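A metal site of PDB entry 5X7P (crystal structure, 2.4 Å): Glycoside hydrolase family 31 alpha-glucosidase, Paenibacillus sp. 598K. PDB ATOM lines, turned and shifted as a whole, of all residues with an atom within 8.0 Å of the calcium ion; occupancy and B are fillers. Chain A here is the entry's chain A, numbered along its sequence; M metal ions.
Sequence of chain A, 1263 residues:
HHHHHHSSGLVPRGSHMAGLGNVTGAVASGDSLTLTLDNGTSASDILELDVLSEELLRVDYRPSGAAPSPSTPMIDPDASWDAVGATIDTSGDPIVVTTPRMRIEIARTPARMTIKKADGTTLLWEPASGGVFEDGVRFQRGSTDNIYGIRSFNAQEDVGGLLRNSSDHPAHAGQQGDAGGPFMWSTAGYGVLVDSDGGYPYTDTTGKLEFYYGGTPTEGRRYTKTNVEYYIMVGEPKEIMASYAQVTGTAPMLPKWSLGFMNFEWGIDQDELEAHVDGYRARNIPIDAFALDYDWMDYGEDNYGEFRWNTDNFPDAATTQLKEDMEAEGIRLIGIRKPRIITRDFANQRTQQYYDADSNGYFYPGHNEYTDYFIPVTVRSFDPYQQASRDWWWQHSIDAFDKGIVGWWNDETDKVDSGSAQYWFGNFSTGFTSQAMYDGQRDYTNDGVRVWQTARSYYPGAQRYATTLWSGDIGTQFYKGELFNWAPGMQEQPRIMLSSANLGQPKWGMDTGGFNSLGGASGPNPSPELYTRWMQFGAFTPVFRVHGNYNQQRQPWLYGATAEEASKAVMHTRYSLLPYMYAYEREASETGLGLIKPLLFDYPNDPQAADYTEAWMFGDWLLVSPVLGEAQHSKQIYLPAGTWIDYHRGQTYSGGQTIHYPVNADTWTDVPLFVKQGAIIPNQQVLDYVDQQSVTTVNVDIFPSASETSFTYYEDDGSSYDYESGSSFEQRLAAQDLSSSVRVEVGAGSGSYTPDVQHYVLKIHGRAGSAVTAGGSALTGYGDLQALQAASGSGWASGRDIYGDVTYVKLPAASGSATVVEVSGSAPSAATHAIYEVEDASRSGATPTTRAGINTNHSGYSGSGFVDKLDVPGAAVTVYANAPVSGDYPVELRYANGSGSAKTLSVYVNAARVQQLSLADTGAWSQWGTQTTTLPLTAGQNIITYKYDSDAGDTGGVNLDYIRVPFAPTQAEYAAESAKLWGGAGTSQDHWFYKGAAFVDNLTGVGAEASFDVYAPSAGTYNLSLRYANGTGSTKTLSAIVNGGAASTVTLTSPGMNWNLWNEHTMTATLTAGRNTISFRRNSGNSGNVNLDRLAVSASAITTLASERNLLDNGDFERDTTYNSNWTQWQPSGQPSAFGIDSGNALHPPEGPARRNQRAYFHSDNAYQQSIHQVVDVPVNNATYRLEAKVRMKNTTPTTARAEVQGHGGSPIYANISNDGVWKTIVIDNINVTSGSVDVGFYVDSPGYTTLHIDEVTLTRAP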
ATOM      1  N   GLN A 786     -25.935  -7.636  10.964  1.00  0.00           N
ATOM      2  CA  GLN A 786     -25.451  -6.280  10.784  1.00  0.00           C
ATOM      3  C   GLN A 786     -25.482  -5.802   9.289  1.00  0.00           C
ATOM      4  O   GLN A 786     -26.117  -4.771   8.968  1.00  0.00           O
ATOM      5  CB  GLN A 786     -24.041  -6.146  11.410  1.00  0.00           C
ATOM      6  CG  GLN A 786     -23.799  -4.798  12.082  1.00  0.00           C
ATOM      7  CD  GLN A 786     -23.936  -3.633  11.098  1.00  0.00           C
ATOM      8  OE1 GLN A 786     -23.044  -3.400  10.267  1.00  0.00           O
ATOM      9  NE2 GLN A 786     -25.052  -2.887  11.189  1.00  0.00           N
ATOM     10  N   ILE A 835     -22.387 -11.017  19.287  1.00  0.00           N
ATOM     11  CA  ILE A 835     -21.915  -9.658  19.247  1.00  0.00           C
ATOM     12  C   ILE A 835     -23.048  -8.726  19.627  1.00  0.00           C
ATOM     13  O   ILE A 835     -24.066  -8.666  18.952  1.00  0.00           O
ATOM     14  CB  ILE A 835     -21.269  -9.310  17.887  1.00  0.00           C
ATOM     15  CG1 ILE A 835     -20.639  -7.916  17.929  1.00  0.00           C
ATOM     16  CG2 ILE A 835     -22.270  -9.391  16.723  1.00  0.00           C
ATOM     17  CD1 ILE A 835     -19.701  -7.614  16.771  1.00  0.00           C
ATOM     18  N   TYR A 836     -22.861  -7.969  20.710  1.00  0.00           N
ATOM     19  CA  TYR A 836     -23.752  -6.889  21.021  1.00  0.00           C
ATOM     20  C   TYR A 836     -23.073  -5.525  20.744  1.00  0.00           C
ATOM     21  O   TYR A 836     -22.089  -5.159  21.406  1.00  0.00           O
ATOM     22  CB  TYR A 836     -24.193  -7.005  22.466  1.00  0.00           C
ATOM     23  CG  TYR A 836     -24.812  -8.329  22.818  1.00  0.00           C
ATOM     24  CD1 TYR A 836     -23.996  -9.411  23.178  1.00  0.00           C
ATOM     25  CD2 TYR A 836     -26.205  -8.516  22.831  1.00  0.00           C
ATOM     26  CE1 TYR A 836     -24.539 -10.632  23.518  1.00  0.00           C
ATOM     27  CE2 TYR A 836     -26.769  -9.773  23.146  1.00  0.00           C
ATOM     28  CZ  TYR A 836     -25.918 -10.811  23.507  1.00  0.00           C
ATOM     29  OH  TYR A 836     -26.355 -12.042  23.864  1.00  0.00           O
ATOM     30  N   GLU A 837     -23.607  -4.796  19.754  1.00  0.00           N
ATOM     31  CA  GLU A 837     -23.200  -3.438  19.468  1.00  0.00           C
ATOM     32  C   GLU A 837     -23.793  -2.515  20.540  1.00  0.00           C
ATOM     33  O   GLU A 837     -25.025  -2.428  20.643  1.00  0.00           O
ATOM     34  CB  GLU A 837     -23.750  -3.000  18.105  1.00  0.00           C
ATOM     35  CG  GLU A 837     -23.211  -3.769  16.893  1.00  0.00           C
ATOM     36  CD  GLU A 837     -21.710  -3.554  16.610  1.00  0.00           C
ATOM     37  OE1 GLU A 837     -21.089  -2.643  17.232  1.00  0.00           O
ATOM     38  OE2 GLU A 837     -21.153  -4.302  15.770  1.00  0.00           O
ATOM     39  N   VAL A 838     -22.934  -1.817  21.288  1.00  0.00           N
ATOM     40  CA  VAL A 838     -23.380  -1.091  22.480  1.00  0.00           C
ATOM     41  C   VAL A 838     -24.156   0.170  22.192  1.00  0.00           C
ATOM     42  O   VAL A 838     -24.872   0.665  23.036  1.00  0.00           O
ATOM     43  CB  VAL A 838     -22.254  -0.777  23.467  1.00  0.00           C
ATOM     44  CG1 VAL A 838     -21.843  -2.073  24.153  1.00  0.00           C
ATOM     45  CG2 VAL A 838     -21.071  -0.104  22.769  1.00  0.00           C
ATOM     46  N   GLU A 839     -24.047   0.662  20.976  1.00  0.00           N
ATOM     47  CA  GLU A 839     -24.915   1.760  20.556  1.00  0.00           C
ATOM     48  C   GLU A 839     -26.409   1.327  20.454  1.00  0.00           C
ATOM     49  O   GLU A 839     -27.286   2.157  20.563  1.00  0.00           O
ATOM     50  CB  GLU A 839     -24.415   2.359  19.225  1.00  0.00           C
ATOM     51  CG  GLU A 839     -24.446   1.427  18.009  1.00  0.00           C
ATOM     52  CD  GLU A 839     -23.191   0.642  17.816  1.00  0.00           C
ATOM     53  OE1 GLU A 839     -22.447   0.402  18.814  1.00  0.00           O
ATOM     54  OE2 GLU A 839     -22.951   0.204  16.664  1.00  0.00           O
ATOM     55  N   ASP A 840     -26.672   0.034  20.263  1.00  0.00           N
ATOM     56  CA  ASP A 840     -28.031  -0.522  20.405  1.00  0.00           C
ATOM     57  C   ASP A 840     -28.407  -0.813  21.861  1.00  0.00           C
ATOM     58  O   ASP A 840     -29.598  -1.050  22.132  1.00  0.00           O
ATOM     59  CB  ASP A 840     -28.190  -1.821  19.594  1.00  0.00           C
ATOM     60  CG  ASP A 840     -27.963  -1.618  18.086  1.00  0.00           C
ATOM     61  OD1 ASP A 840     -28.050  -0.473  17.626  1.00  0.00           O
ATOM     62  OD2 ASP A 840     -27.685  -2.605  17.372  1.00  0.00           O
ATOM     63  N   ASN A 855     -22.474   7.868  18.882  1.00  0.00           N
ATOM     64  CA  ASN A 855     -21.770   8.730  17.923  1.00  0.00           C
ATOM     65  C   ASN A 855     -21.115   7.950  16.767  1.00  0.00           C
ATOM     66  O   ASN A 855     -20.960   6.736  16.829  1.00  0.00           O
ATOM     67  CB  ASN A 855     -20.742   9.593  18.659  1.00  0.00           C
ATOM     68  CG  ASN A 855     -20.742  11.047  18.181  1.00  0.00           C
ATOM     69  OD1 ASN A 855     -20.840  11.304  16.972  1.00  0.00           O
ATOM     70  ND2 ASN A 855     -20.619  11.984  19.125  1.00  0.00           N
ATOM     71  N   GLY A 860     -13.743   3.593  11.901  1.00  0.00           N
ATOM     72  CA  GLY A 860     -13.292   2.254  12.286  1.00  0.00           C
ATOM     73  C   GLY A 860     -14.263   1.431  13.134  1.00  0.00           C
ATOM     74  O   GLY A 860     -13.998   0.258  13.397  1.00  0.00           O
ATOM     75  N   TYR A 861     -15.361   2.030  13.588  1.00  0.00           N
ATOM     76  CA  TYR A 861     -16.347   1.318  14.423  1.00  0.00           C
ATOM     77  C   TYR A 861     -17.026   0.184  13.635  1.00  0.00           C
ATOM     78  O   TYR A 861     -17.110   0.226  12.401  1.00  0.00           O
ATOM     79  CB  TYR A 861     -17.408   2.255  15.038  1.00  0.00           C
ATOM     80  CG  TYR A 861     -18.188   3.031  14.012  1.00  0.00           C
ATOM     81  CD1 TYR A 861     -19.264   2.450  13.331  1.00  0.00           C
ATOM     82  CD2 TYR A 861     -17.838   4.353  13.696  1.00  0.00           C
ATOM     83  CE1 TYR A 861     -19.963   3.161  12.365  1.00  0.00           C
ATOM     84  CE2 TYR A 861     -18.521   5.078  12.736  1.00  0.00           C
ATOM     85  CZ  TYR A 861     -19.585   4.470  12.070  1.00  0.00           C
ATOM     86  OH  TYR A 861     -20.263   5.164  11.119  1.00  0.00           O
ATOM     87  N   SER A 862     -17.503  -0.805  14.374  1.00  0.00           N
ATOM     88  CA  SER A 862     -18.469  -1.799  13.879  1.00  0.00           C
ATOM     89  C   SER A 862     -19.940  -1.321  14.074  1.00  0.00           C
ATOM     90  O   SER A 862     -20.248  -0.479  14.933  1.00  0.00           O
ATOM     91  CB  SER A 862     -18.226  -3.094  14.620  1.00  0.00           C
ATOM     92  OG  SER A 862     -19.049  -4.080  14.118  1.00  0.00           O
ATOM     93  N   GLY A 863     -20.827  -1.869  13.259  1.00  0.00           N
ATOM     94  CA  GLY A 863     -22.244  -1.524  13.318  1.00  0.00           C
ATOM     95  C   GLY A 863     -22.532  -0.111  12.885  1.00  0.00           C
ATOM     96  O   GLY A 863     -21.887   0.410  11.993  1.00  0.00           O
ATOM     97  N   SER A 864     -23.483   0.526  13.562  1.00  0.00           N
ATOM     98  CA  SER A 864     -23.936   1.848  13.187  1.00  0.00           C
ATOM     99  C   SER A 864     -23.198   2.949  13.947  1.00  0.00           C
ATOM    100  O   SER A 864     -23.406   4.134  13.653  1.00  0.00           O
ATOM    101  CB  SER A 864     -25.452   1.931  13.438  1.00  0.00           C
ATOM    102  OG  SER A 864     -25.780   1.513  14.765  1.00  0.00           O
ATOM    103  N   GLY A 865     -22.349   2.595  14.907  1.00  0.00           N
ATOM    104  CA  GLY A 865     -21.685   3.598  15.709  1.00  0.00           C
ATOM    105  C   GLY A 865     -20.896   3.049  16.881  1.00  0.00           C
ATOM    106  O   GLY A 865     -20.407   1.932  16.860  1.00  0.00           O
ATOM    107  N   PHE A 866     -20.777   3.869  17.903  1.00  0.00           N
ATOM    108  CA  PHE A 866     -20.151   3.467  19.160  1.00  0.00           C
ATOM    109  C   PHE A 866     -20.742   4.316  20.283  1.00  0.00           C
ATOM    110  O   PHE A 866     -21.622   5.131  20.014  1.00  0.00           O
ATOM    111  CB  PHE A 866     -18.662   3.664  19.062  1.00  0.00           C
ATOM    112  CG  PHE A 866     -18.271   5.033  18.615  1.00  0.00           C
ATOM    113  CD1 PHE A 866     -18.124   5.324  17.263  1.00  0.00           C
ATOM    114  CD2 PHE A 866     -17.986   6.024  19.556  1.00  0.00           C
ATOM    115  CE1 PHE A 866     -17.729   6.589  16.859  1.00  0.00           C
ATOM    116  CE2 PHE A 866     -17.562   7.295  19.145  1.00  0.00           C
ATOM    117  CZ  PHE A 866     -17.451   7.578  17.794  1.00  0.00           C
ATOM    118  N   VAL A 867     -20.273   4.158  21.517  1.00  0.00           N
ATOM    119  CA  VAL A 867     -20.862   4.873  22.611  1.00  0.00           C
ATOM    120  C   VAL A 867     -19.830   5.837  23.206  1.00  0.00           C
ATOM    121  O   VAL A 867     -18.728   5.411  23.532  1.00  0.00           O
ATOM    122  CB  VAL A 867     -21.400   3.872  23.655  1.00  0.00           C
ATOM    123  CG1 VAL A 867     -21.743   4.568  24.950  1.00  0.00           C
ATOM    124  CG2 VAL A 867     -22.634   3.166  23.093  1.00  0.00           C
ATOM    125  N   ARG A 894     -14.749  -4.182  22.783  1.00  0.00           N
ATOM    126  CA  ARG A 894     -14.024  -3.380  21.807  1.00  0.00           C
ATOM    127  C   ARG A 894     -14.208  -1.905  22.140  1.00  0.00           C
ATOM    128  O   ARG A 894     -15.362  -1.405  22.223  1.00  0.00           O
ATOM    129  CB  ARG A 894     -14.488  -3.669  20.372  1.00  0.00           C
ATOM    130  CG  ARG A 894     -13.561  -3.043  19.323  1.00  0.00           C
ATOM    131  CD  ARG A 894     -13.533  -3.802  18.015  1.00  0.00           C
ATOM    132  NE  ARG A 894     -12.470  -3.358  17.113  1.00  0.00           N
ATOM    133  CZ  ARG A 894     -12.581  -2.402  16.173  1.00  0.00           C
ATOM    134  NH1 ARG A 894     -13.702  -1.684  16.001  1.00  0.00           N
ATOM    135  NH2 ARG A 894     -11.521  -2.123  15.425  1.00  0.00           N
ATOM    136  N   TRP A 928      -8.821   1.280  17.515  1.00  0.00           N
ATOM    137  CA  TRP A 928      -9.637   0.470  18.426  1.00  0.00           C
ATOM    138  C   TRP A 928      -8.803  -0.679  18.970  1.00  0.00           C
ATOM    139  O   TRP A 928      -7.898  -1.166  18.286  1.00  0.00           O
ATOM    140  CB  TRP A 928     -10.889  -0.063  17.682  1.00  0.00           C
ATOM    141  CG  TRP A 928     -11.772   1.044  17.119  1.00  0.00           C
ATOM    142  CD1 TRP A 928     -11.657   1.647  15.895  1.00  0.00           C
ATOM    143  CD2 TRP A 928     -12.879   1.693  17.793  1.00  0.00           C
ATOM    144  NE1 TRP A 928     -12.621   2.643  15.761  1.00  0.00           N
ATOM    145  CE2 TRP A 928     -13.374   2.690  16.905  1.00  0.00           C
ATOM    146  CE3 TRP A 928     -13.486   1.535  19.045  1.00  0.00           C
ATOM    147  CZ2 TRP A 928     -14.456   3.532  17.240  1.00  0.00           C
ATOM    148  CZ3 TRP A 928     -14.572   2.353  19.379  1.00  0.00           C
ATOM    149  CH2 TRP A 928     -15.046   3.352  18.478  1.00  0.00           C
ATOM    150  N   LEU A 960     -16.885   3.019  23.450  1.00  0.00           N
ATOM    151  CA  LEU A 960     -17.087   1.574  23.405  1.00  0.00           C
ATOM    152  C   LEU A 960     -17.836   1.199  22.157  1.00  0.00           C
ATOM    153  O   LEU A 960     -18.775   1.897  21.742  1.00  0.00           O
ATOM    154  CB  LEU A 960     -17.871   1.151  24.638  1.00  0.00           C
ATOM    155  CG  LEU A 960     -17.265   1.460  26.009  1.00  0.00           C
ATOM    156  CD1 LEU A 960     -18.189   0.902  27.092  1.00  0.00           C
ATOM    157  CD2 LEU A 960     -15.831   0.947  26.219  1.00  0.00           C
ATOM    158  N   ASP A 961     -17.401   0.117  21.521  1.00  0.00           N
ATOM    159  CA  ASP A 961     -17.962  -0.212  20.221  1.00  0.00           C
ATOM    160  C   ASP A 961     -18.914  -1.409  20.247  1.00  0.00           C
ATOM    161  O   ASP A 961     -19.995  -1.369  19.648  1.00  0.00           O
ATOM    162  CB  ASP A 961     -16.824  -0.461  19.243  1.00  0.00           C
ATOM    163  CG  ASP A 961     -17.317  -0.704  17.843  1.00  0.00           C
ATOM    164  OD1 ASP A 961     -18.450  -0.280  17.489  1.00  0.00           O
ATOM    165  OD2 ASP A 961     -16.540  -1.329  17.083  1.00  0.00           O
ATOM    166  N   TYR A 962     -18.465  -2.485  20.898  1.00  0.00           N
ATOM    167  CA  TYR A 962     -19.280  -3.687  21.073  1.00  0.00           C
ATOM    168  C   TYR A 962     -18.707  -4.557  22.165  1.00  0.00           C
ATOM    169  O   TYR A 962     -17.603  -4.291  22.655  1.00  0.00           O
ATOM    170  CB  TYR A 962     -19.397  -4.522  19.771  1.00  0.00           C
ATOM    171  CG  TYR A 962     -18.098  -5.088  19.148  1.00  0.00           C
ATOM    172  CD1 TYR A 962     -17.339  -6.078  19.791  1.00  0.00           C
ATOM    173  CD2 TYR A 962     -17.663  -4.691  17.860  1.00  0.00           C
ATOM    174  CE1 TYR A 962     -16.199  -6.624  19.217  1.00  0.00           C
ATOM    175  CE2 TYR A 962     -16.526  -5.251  17.263  1.00  0.00           C
ATOM    176  CZ  TYR A 962     -15.789  -6.218  17.961  1.00  0.00           C
ATOM    177  OH  TYR A 962     -14.621  -6.787  17.430  1.00  0.00           O
ATOM    178  N   ILE A 963     -19.467  -5.589  22.555  1.00  0.00           N
ATOM    179  CA  ILE A 963     -18.888  -6.695  23.290  1.00  0.00           C
ATOM    180  C   ILE A 963     -19.218  -7.993  22.592  1.00  0.00           C
ATOM    181  O   ILE A 963     -20.200  -8.054  21.817  1.00  0.00           O
ATOM    182  CB  ILE A 963     -19.324  -6.790  24.772  1.00  0.00           C
ATOM    183  CG1 ILE A 963     -20.855  -6.940  24.905  1.00  0.00           C
ATOM    184  CG2 ILE A 963     -18.814  -5.561  25.519  1.00  0.00           C
ATOM    185  CD1 ILE A 963     -21.305  -7.436  26.259  1.00  0.00           C
HETATM  186 CA    CA M   1     -20.629  -0.494  17.399  1.00  0.00          CA
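The backbone carbonyl oxygen (O) of Asp 961 lies close to the backbone NH (N) of Val 838 (3.4 Å).
OD2 of Asp 961 is in salt-bridge range of NH1 of Arg 894, at 3.1 Å.
N of Ser 864 lies close to OE2 of Glu 839 (3.2 Å).
The calcium ion is bound by the side-chain carboxylate (OD1) of Asp 961 (2.2 Å), the side-chain carboxylate (OE1) of Glu 837 (2.2 Å), the side-chain carboxylate (OE1) of Glu 839 (2.5 Å), the backbone carbonyl oxygen (O) of Gly 865 (2.5 Å), the backbone carbonyl oxygen (O) of Asp 961 (2.5 Å), the backbone carbonyl oxygen (O) of Ser 862 (2.5 Å) and the side-chain carboxylate (OE2) of Glu 839 (2.5 Å).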
